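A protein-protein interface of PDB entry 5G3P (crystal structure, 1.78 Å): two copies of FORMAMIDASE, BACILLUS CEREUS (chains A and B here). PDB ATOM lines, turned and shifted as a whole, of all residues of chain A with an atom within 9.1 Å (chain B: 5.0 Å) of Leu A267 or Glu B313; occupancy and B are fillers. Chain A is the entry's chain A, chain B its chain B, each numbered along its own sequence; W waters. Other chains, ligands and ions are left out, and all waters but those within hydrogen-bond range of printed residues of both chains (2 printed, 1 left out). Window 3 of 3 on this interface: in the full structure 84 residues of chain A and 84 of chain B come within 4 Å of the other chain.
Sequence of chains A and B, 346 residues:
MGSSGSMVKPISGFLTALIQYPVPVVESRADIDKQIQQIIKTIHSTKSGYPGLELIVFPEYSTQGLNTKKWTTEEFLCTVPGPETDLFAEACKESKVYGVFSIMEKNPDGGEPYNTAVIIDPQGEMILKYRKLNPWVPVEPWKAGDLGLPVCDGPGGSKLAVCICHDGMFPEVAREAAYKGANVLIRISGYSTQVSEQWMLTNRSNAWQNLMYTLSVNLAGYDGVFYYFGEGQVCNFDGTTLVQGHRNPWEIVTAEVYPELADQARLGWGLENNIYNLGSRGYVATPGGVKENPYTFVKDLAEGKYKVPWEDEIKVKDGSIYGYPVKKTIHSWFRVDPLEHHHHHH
O of Leu A267 sits at hydrogen-bond distance from N of Lys B315, 2.9 Å away.
The backbone carbonyl oxygen of Leu A211 is in hydrogen-bond range of the guanidinium group of Arg A266, at 3.0 Å. The backbone carbonyl oxygen (O) of Arg A266 lies within hydrogen-bond range of the side-chain amide nitrogen (ND2) of Asn A273 (2.9 Å).
Arg A266 touches Trp B310 (NH1 to CH2, 3.7 Å). Ile B314 touches Arg A266. CD2 of Leu A267 touches CD1 of Trp B310, at 3.8 Å. Glu B313 touches Leu A267 (CB to CD2, 3.8 Å). O of Leu A267 touches CA of Ile B314, at 3.6 Å. Gly A268 touches Val B316. CA of Gly A270 touches CG1 of Val B316 (3.9 Å). Trp B310 touches Ile A275 (CZ2 to CG1, 3.8 Å). OE2 of Glu B311 touches CE1 of Tyr A276, at 3.7 Å. Ile B314 touches Tyr A276.
Ala A262 touches none of the printed residues of chain B. Of the printed residues of chain B, Arg A266 touches Trp B310 and Ile B314. Leu A267 touches just these residues of chain B: Trp B310, Glu B313, Ile B314 and Lys B315. Of the printed residues of chain B, Gly A270 touches Val B316 (3.9 Å). Of the printed residues of chain B, Tyr A276 touches Glu B311 and Ile B314. Glu B313 touches just one residue of chain A: Leu A267. The nearest residue of chain B that does not touch Leu A267 is Val B316 (4.4 Å). The nearest residue of chain A that does not touch Glu B313 is Gly A268 (6.0 Å).
Along chain B the printed residues that touch a printed residue of chain A span positions 310 to 316. Hydrophobic or aromatic side chains of chain A that line the printed part of chain B: Leu A267, Ile A275 and Tyr A276. Among the printed residues, no Asp or Glu carboxylate lies within 4 Å of a Lys or Arg side-chain nitrogen of the other chain.
No position is printed for both chains.
Water W1 lies within hydrogen-bond range of the backbone carbonyl oxygen (O) of Val B316 (2.7 Å), the backbone carbonyl oxygen (O) of Trp A269 (3.0 Å) and the side-chain amide nitrogen (ND2) of Asn A273 (3.4 Å). Water W2 lies within hydrogen-bond range of the side-chain amide oxygen of Asn A273 (2.7 Å), the indole nitrogen of Trp B310 (2.8 Å) and the backbone carbonyl oxygen of Arg A266 (2.8 Å).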
ATOM      1  N   LEU A 211     -25.613  15.959  28.636  1.00  0.00           N
ATOM      2  CA  LEU A 211     -24.884  14.983  27.803  1.00  0.00           C
ATOM      3  C   LEU A 211     -23.385  15.120  28.035  1.00  0.00           C
ATOM      4  O   LEU A 211     -22.601  15.356  27.126  1.00  0.00           O
ATOM      5  CB  LEU A 211     -25.262  15.138  26.333  1.00  0.00           C
ATOM      6  CG  LEU A 211     -26.720  14.748  26.043  1.00  0.00           C
ATOM      7  CD1 LEU A 211     -27.095  15.102  24.624  1.00  0.00           C
ATOM      8  CD2 LEU A 211     -26.948  13.255  26.250  1.00  0.00           C
ATOM      9  N   GLU A 260     -15.487  11.725  23.145  1.00  0.00           N
ATOM     10  CA  GLU A 260     -16.054  11.788  21.816  1.00  0.00           C
ATOM     11  C   GLU A 260     -17.485  11.239  21.739  1.00  0.00           C
ATOM     12  O   GLU A 260     -18.287  11.721  20.926  1.00  0.00           O
ATOM     13  CB  GLU A 260     -15.100  11.108  20.813  1.00  0.00           C
ATOM     14  CG  GLU A 260     -15.604  11.117  19.393  1.00  0.00           C
ATOM     15  CD  GLU A 260     -15.769  12.503  18.811  1.00  0.00           C
ATOM     16  OE1 GLU A 260     -15.231  13.456  19.414  1.00  0.00           O
ATOM     17  OE2 GLU A 260     -16.433  12.634  17.750  1.00  0.00           O
ATOM     18  N   LEU A 261     -17.820  10.270  22.589  1.00  0.00           N
ATOM     19  CA  LEU A 261     -19.194   9.758  22.644  1.00  0.00           C
ATOM     20  C   LEU A 261     -20.209  10.799  23.131  1.00  0.00           C
ATOM     21  O   LEU A 261     -21.339  10.865  22.628  1.00  0.00           O
ATOM     22  CB  LEU A 261     -19.293   8.533  23.538  1.00  0.00           C
ATOM     23  CG  LEU A 261     -18.540   7.314  23.012  1.00  0.00           C
ATOM     24  CD1 LEU A 261     -18.702   6.238  24.074  1.00  0.00           C
ATOM     25  CD2 LEU A 261     -19.029   6.840  21.665  1.00  0.00           C
ATOM     26  N   ALA A 262     -19.797  11.621  24.076  1.00  0.00           N
ATOM     27  CA  ALA A 262     -20.630  12.730  24.524  1.00  0.00           C
ATOM     28  C   ALA A 262     -20.742  13.803  23.448  1.00  0.00           C
ATOM     29  O   ALA A 262     -21.857  14.257  23.167  1.00  0.00           O
ATOM     30  CB  ALA A 262     -20.082  13.324  25.808  1.00  0.00           C
ATOM     31  N   ASP A 263     -19.625  14.179  22.823  1.00  0.00           N
ATOM     32  CA  ASP A 263     -19.678  15.119  21.696  1.00  0.00           C
ATOM     33  C   ASP A 263     -20.628  14.596  20.596  1.00  0.00           C
ATOM     34  O   ASP A 263     -21.409  15.357  20.039  1.00  0.00           O
ATOM     35  CB  ASP A 263     -18.309  15.364  21.062  1.00  0.00           C
ATOM     36  CG  ASP A 263     -17.325  16.045  22.002  1.00  0.00           C
ATOM     37  OD1 ASP A 263     -17.728  16.589  23.077  1.00  0.00           O
ATOM     38  OD2 ASP A 263     -16.140  16.039  21.653  1.00  0.00           O
ATOM     39  N   GLN A 264     -20.522  13.303  20.271  1.00  0.00           N
ATOM     40  CA  GLN A 264     -21.351  12.700  19.228  1.00  0.00           C
ATOM     41  C   GLN A 264     -22.839  12.693  19.542  1.00  0.00           C
ATOM     42  O   GLN A 264     -23.651  12.920  18.656  1.00  0.00           O
ATOM     43  CB  GLN A 264     -20.884  11.279  18.912  1.00  0.00           C
ATOM     44  CG  GLN A 264     -19.650  11.309  18.063  1.00  0.00           C
ATOM     45  CD  GLN A 264     -18.932   9.964  18.017  1.00  0.00           C
ATOM     46  OE1 GLN A 264     -19.527   8.927  18.253  1.00  0.00           O
ATOM     47  NE2 GLN A 264     -17.648   9.988  17.696  1.00  0.00           N
ATOM     48  N   ALA A 265     -23.186  12.464  20.794  1.00  0.00           N
ATOM     49  CA  ALA A 265     -24.563  12.544  21.222  1.00  0.00           C
ATOM     50  C   ALA A 265     -25.070  13.984  21.102  1.00  0.00           C
ATOM     51  O   ALA A 265     -26.192  14.223  20.618  1.00  0.00           O
ATOM     52  CB  ALA A 265     -24.730  12.031  22.652  1.00  0.00           C
ATOM     53  N   ARG A 266     -24.244  14.939  21.510  1.00  0.00           N
ATOM     54  CA  ARG A 266     -24.595  16.342  21.346  1.00  0.00           C
ATOM     55  C   ARG A 266     -24.829  16.721  19.877  1.00  0.00           C
ATOM     56  O   ARG A 266     -25.707  17.525  19.586  1.00  0.00           O
ATOM     57  CB  ARG A 266     -23.518  17.265  21.953  1.00  0.00           C
ATOM     58  CG  ARG A 266     -23.510  17.205  23.468  1.00  0.00           C
ATOM     59  CD  ARG A 266     -22.231  17.798  24.011  1.00  0.00           C
ATOM     60  NE  ARG A 266     -22.278  17.861  25.473  1.00  0.00           N
ATOM     61  CZ  ARG A 266     -21.428  18.543  26.221  1.00  0.00           C
ATOM     62  NH1 ARG A 266     -20.430  19.225  25.675  1.00  0.00           N
ATOM     63  NH2 ARG A 266     -21.590  18.565  27.537  1.00  0.00           N
ATOM     64  N   LEU A 267     -24.023  16.184  18.961  1.00  0.00           N
ATOM     65  CA  LEU A 267     -24.222  16.488  17.555  1.00  0.00           C
ATOM     66  C   LEU A 267     -25.368  15.684  16.946  1.00  0.00           C
ATOM     67  O   LEU A 267     -26.021  16.181  16.030  1.00  0.00           O
ATOM     68  CB  LEU A 267     -22.953  16.260  16.727  1.00  0.00           C
ATOM     69  CG  LEU A 267     -21.709  17.052  17.119  1.00  0.00           C
ATOM     70  CD1 LEU A 267     -20.641  16.838  16.032  1.00  0.00           C
ATOM     71  CD2 LEU A 267     -21.974  18.539  17.318  1.00  0.00           C
ATOM     72  N   GLY A 268     -25.625  14.492  17.468  1.00  0.00           N
ATOM     73  CA  GLY A 268     -26.463  13.512  16.801  1.00  0.00           C
ATOM     74  C   GLY A 268     -27.858  13.331  17.357  1.00  0.00           C
ATOM     75  O   GLY A 268     -28.791  13.063  16.599  1.00  0.00           O
ATOM     76  N   TRP A 269     -28.013  13.457  18.667  1.00  0.00           N
ATOM     77  CA  TRP A 269     -29.309  13.167  19.291  1.00  0.00           C
ATOM     78  C   TRP A 269     -30.422  14.102  18.785  1.00  0.00           C
ATOM     79  O   TRP A 269     -30.183  15.279  18.510  1.00  0.00           O
ATOM     80  CB  TRP A 269     -29.225  13.219  20.817  1.00  0.00           C
ATOM     81  CG  TRP A 269     -28.658  11.958  21.458  1.00  0.00           C
ATOM     82  CD1 TRP A 269     -27.760  11.077  20.909  1.00  0.00           C
ATOM     83  CD2 TRP A 269     -28.937  11.480  22.769  1.00  0.00           C
ATOM     84  NE1 TRP A 269     -27.483  10.078  21.789  1.00  0.00           N
ATOM     85  CE2 TRP A 269     -28.181  10.307  22.952  1.00  0.00           C
ATOM     86  CE3 TRP A 269     -29.749  11.941  23.823  1.00  0.00           C
ATOM     87  CZ2 TRP A 269     -28.236   9.566  24.125  1.00  0.00           C
ATOM     88  CZ3 TRP A 269     -29.814  11.203  24.974  1.00  0.00           C
ATOM     89  CH2 TRP A 269     -29.061  10.031  25.126  1.00  0.00           C
ATOM     90  N   GLY A 270     -31.598  13.530  18.601  1.00  0.00           N
ATOM     91  CA  GLY A 270     -32.834  14.282  18.322  1.00  0.00           C
ATOM     92  C   GLY A 270     -33.589  14.449  19.630  1.00  0.00           C
ATOM     93  O   GLY A 270     -33.401  15.420  20.337  1.00  0.00           O
ATOM     94  N   ASN A 273     -32.008  15.961  23.177  1.00  0.00           N
ATOM     95  CA  ASN A 273     -30.853  16.816  22.987  1.00  0.00           C
ATOM     96  C   ASN A 273     -31.073  18.125  23.744  1.00  0.00           C
ATOM     97  O   ASN A 273     -31.297  19.188  23.171  1.00  0.00           O
ATOM     98  CB  ASN A 273     -30.558  17.049  21.513  1.00  0.00           C
ATOM     99  CG  ASN A 273     -29.118  17.505  21.290  1.00  0.00           C
ATOM    100  OD1 ASN A 273     -28.534  18.172  22.143  1.00  0.00           O
ATOM    101  ND2 ASN A 273     -28.527  17.101  20.169  1.00  0.00           N
ATOM    102  N   ILE A 275     -29.425  20.060  25.993  1.00  0.00           N
ATOM    103  CA  ILE A 275     -28.443  21.155  25.997  1.00  0.00           C
ATOM    104  C   ILE A 275     -28.649  22.101  24.822  1.00  0.00           C
ATOM    105  O   ILE A 275     -28.491  23.317  24.955  1.00  0.00           O
ATOM    106  CB  ILE A 275     -26.979  20.603  26.082  1.00  0.00           C
ATOM    107  CG1 ILE A 275     -25.944  21.709  26.273  1.00  0.00           C
ATOM    108  CG2 ILE A 275     -26.619  19.762  24.856  1.00  0.00           C
ATOM    109  CD1 ILE A 275     -26.007  22.375  27.605  1.00  0.00           C
ATOM    110  N   TYR A 276     -29.058  21.565  23.678  1.00  0.00           N
ATOM    111  CA  TYR A 276     -29.487  22.388  22.567  1.00  0.00           C
ATOM    112  C   TYR A 276     -30.923  22.907  22.734  1.00  0.00           C
ATOM    113  O   TYR A 276     -31.201  24.082  22.487  1.00  0.00           O
ATOM    114  CB  TYR A 276     -29.359  21.592  21.269  1.00  0.00           C
ATOM    115  CG  TYR A 276     -29.924  22.268  20.034  1.00  0.00           C
ATOM    116  CD1 TYR A 276     -29.612  23.602  19.731  1.00  0.00           C
ATOM    117  CD2 TYR A 276     -30.754  21.570  19.156  1.00  0.00           C
ATOM    118  CE1 TYR A 276     -30.134  24.231  18.602  1.00  0.00           C
ATOM    119  CE2 TYR A 276     -31.259  22.178  18.020  1.00  0.00           C
ATOM    120  CZ  TYR A 276     -30.966  23.508  17.757  1.00  0.00           C
ATOM    121  OH  TYR A 276     -31.465  24.093  16.613  1.00  0.00           O
ATOM    122  N   PRO B 309     -21.797  26.306  21.623  1.00  0.00           N
ATOM    123  CA  PRO B 309     -20.680  26.607  20.697  1.00  0.00           C
ATOM    124  C   PRO B 309     -20.534  25.634  19.524  1.00  0.00           C
ATOM    125  O   PRO B 309     -19.834  25.955  18.577  1.00  0.00           O
ATOM    126  CB  PRO B 309     -19.415  26.598  21.590  1.00  0.00           C
ATOM    127  CG  PRO B 309     -19.847  26.209  22.946  1.00  0.00           C
ATOM    128  CD  PRO B 309     -21.357  26.159  23.014  1.00  0.00           C
ATOM    129  N   TRP B 310     -21.201  24.480  19.588  1.00  0.00           N
ATOM    130  CA  TRP B 310     -21.191  23.482  18.513  1.00  0.00           C
ATOM    131  C   TRP B 310     -22.503  23.506  17.679  1.00  0.00           C
ATOM    132  O   TRP B 310     -22.761  22.578  16.912  1.00  0.00           O
ATOM    133  CB  TRP B 310     -20.971  22.078  19.105  1.00  0.00           C
ATOM    134  CG  TRP B 310     -22.024  21.695  20.105  1.00  0.00           C
ATOM    135  CD1 TRP B 310     -23.241  21.101  19.855  1.00  0.00           C
ATOM    136  CD2 TRP B 310     -21.973  21.907  21.517  1.00  0.00           C
ATOM    137  NE1 TRP B 310     -23.943  20.936  21.025  1.00  0.00           N
ATOM    138  CE2 TRP B 310     -23.174  21.403  22.062  1.00  0.00           C
ATOM    139  CE3 TRP B 310     -21.004  22.454  22.385  1.00  0.00           C
ATOM    140  CZ2 TRP B 310     -23.450  21.442  23.418  1.00  0.00           C
ATOM    141  CZ3 TRP B 310     -21.279  22.486  23.750  1.00  0.00           C
ATOM    142  CH2 TRP B 310     -22.487  21.971  24.246  1.00  0.00           C
ATOM    143  N   GLU B 311     -23.324  24.553  17.830  1.00  0.00           N
ATOM    144  CA  GLU B 311     -24.659  24.566  17.228  1.00  0.00           C
ATOM    145  C   GLU B 311     -24.673  24.339  15.711  1.00  0.00           C
ATOM    146  O   GLU B 311     -25.552  23.638  15.216  1.00  0.00           O
ATOM    147  CB  GLU B 311     -25.413  25.863  17.514  1.00  0.00           C
ATOM    148  CG  GLU B 311     -26.914  25.744  17.258  1.00  0.00           C
ATOM    149  CD  GLU B 311     -27.600  27.087  17.243  1.00  0.00           C
ATOM    150  OE1 GLU B 311     -27.420  27.800  16.255  1.00  0.00           O
ATOM    151  OE2 GLU B 311     -28.269  27.432  18.232  1.00  0.00           O
ATOM    152  N   ASP B 312     -23.691  24.888  15.003  1.00  0.00           N
ATOM    153  CA  ASP B 312     -23.615  24.725  13.548  1.00  0.00           C
ATOM    154  C   ASP B 312     -23.464  23.266  13.089  1.00  0.00           C
ATOM    155  O   ASP B 312     -23.814  22.961  11.949  1.00  0.00           O
ATOM    156  CB  ASP B 312     -22.444  25.515  12.947  1.00  0.00           C
ATOM    157  CG  ASP B 312     -22.599  27.014  13.089  1.00  0.00           C
ATOM    158  OD1 ASP B 312     -23.689  27.507  13.481  1.00  0.00           O
ATOM    159  OD2 ASP B 312     -21.604  27.713  12.829  1.00  0.00           O
ATOM    160  N   GLU B 313     -22.939  22.390  13.955  1.00  0.00           N
ATOM    161  CA  GLU B 313     -22.697  20.982  13.620  1.00  0.00           C
ATOM    162  C   GLU B 313     -23.786  20.037  14.106  1.00  0.00           C
ATOM    163  O   GLU B 313     -23.694  18.845  13.869  1.00  0.00           O
ATOM    164  CB  GLU B 313     -21.334  20.535  14.173  1.00  0.00           C
ATOM    165  CG  GLU B 313     -20.143  21.168  13.474  1.00  0.00           C
ATOM    166  CD  GLU B 313     -19.911  22.617  13.848  1.00  0.00           C
ATOM    167  OE1 GLU B 313     -20.032  22.972  15.051  1.00  0.00           O
ATOM    168  OE2 GLU B 313     -19.608  23.430  12.930  1.00  0.00           O
ATOM    169  N   ILE B 314     -24.812  20.555  14.769  1.00  0.00           N
ATOM    170  CA  ILE B 314     -25.918  19.728  15.229  1.00  0.00           C
ATOM    171  C   ILE B 314     -26.698  19.223  13.999  1.00  0.00           C
ATOM    172  O   ILE B 314     -27.062  20.009  13.133  1.00  0.00           O
ATOM    173  CB  ILE B 314     -26.832  20.501  16.215  1.00  0.00           C
ATOM    174  CG1 ILE B 314     -26.049  20.831  17.508  1.00  0.00           C
ATOM    175  CG2 ILE B 314     -28.107  19.716  16.528  1.00  0.00           C
ATOM    176  CD1 ILE B 314     -26.797  21.694  18.515  1.00  0.00           C
ATOM    177  N   LYS B 315     -26.970  17.928  13.964  1.00  0.00           N
ATOM    178  CA  LYS B 315     -27.562  17.269  12.799  1.00  0.00           C
ATOM    179  C   LYS B 315     -29.076  17.341  12.755  1.00  0.00           C
ATOM    180  O   LYS B 315     -29.650  17.406  11.662  1.00  0.00           O
ATOM    181  CB  LYS B 315     -27.114  15.797  12.727  1.00  0.00           C
ATOM    182  CG  LYS B 315     -25.639  15.629  12.386  1.00  0.00           C
ATOM    183  CD  LYS B 315     -25.065  14.255  12.776  1.00  0.00           C
ATOM    184  CE  LYS B 315     -25.586  13.124  11.897  1.00  0.00           C
ATOM    185  NZ  LYS B 315     -25.046  11.774  12.272  1.00  0.00           N
ATOM    186  N   VAL B 316     -29.732  17.316  13.907  1.00  0.00           N
ATOM    187  CA  VAL B 316     -31.181  17.297  13.968  1.00  0.00           C
ATOM    188  C   VAL B 316     -31.677  18.666  14.445  1.00  0.00           C
ATOM    189  O   VAL B 316     -31.616  18.980  15.627  1.00  0.00           O
ATOM    190  CB  VAL B 316     -31.708  16.151  14.850  1.00  0.00           C
ATOM    191  CG1 VAL B 316     -33.234  16.104  14.843  1.00  0.00           C
ATOM    192  CG2 VAL B 316     -31.154  14.832  14.356  1.00  0.00           C
HETATM  193  O   HOH W   1     -31.048  18.133  18.138  1.00  0.00           O
HETATM  194  O   HOH W   2     -26.320  19.587  21.343  1.00  0.00           O
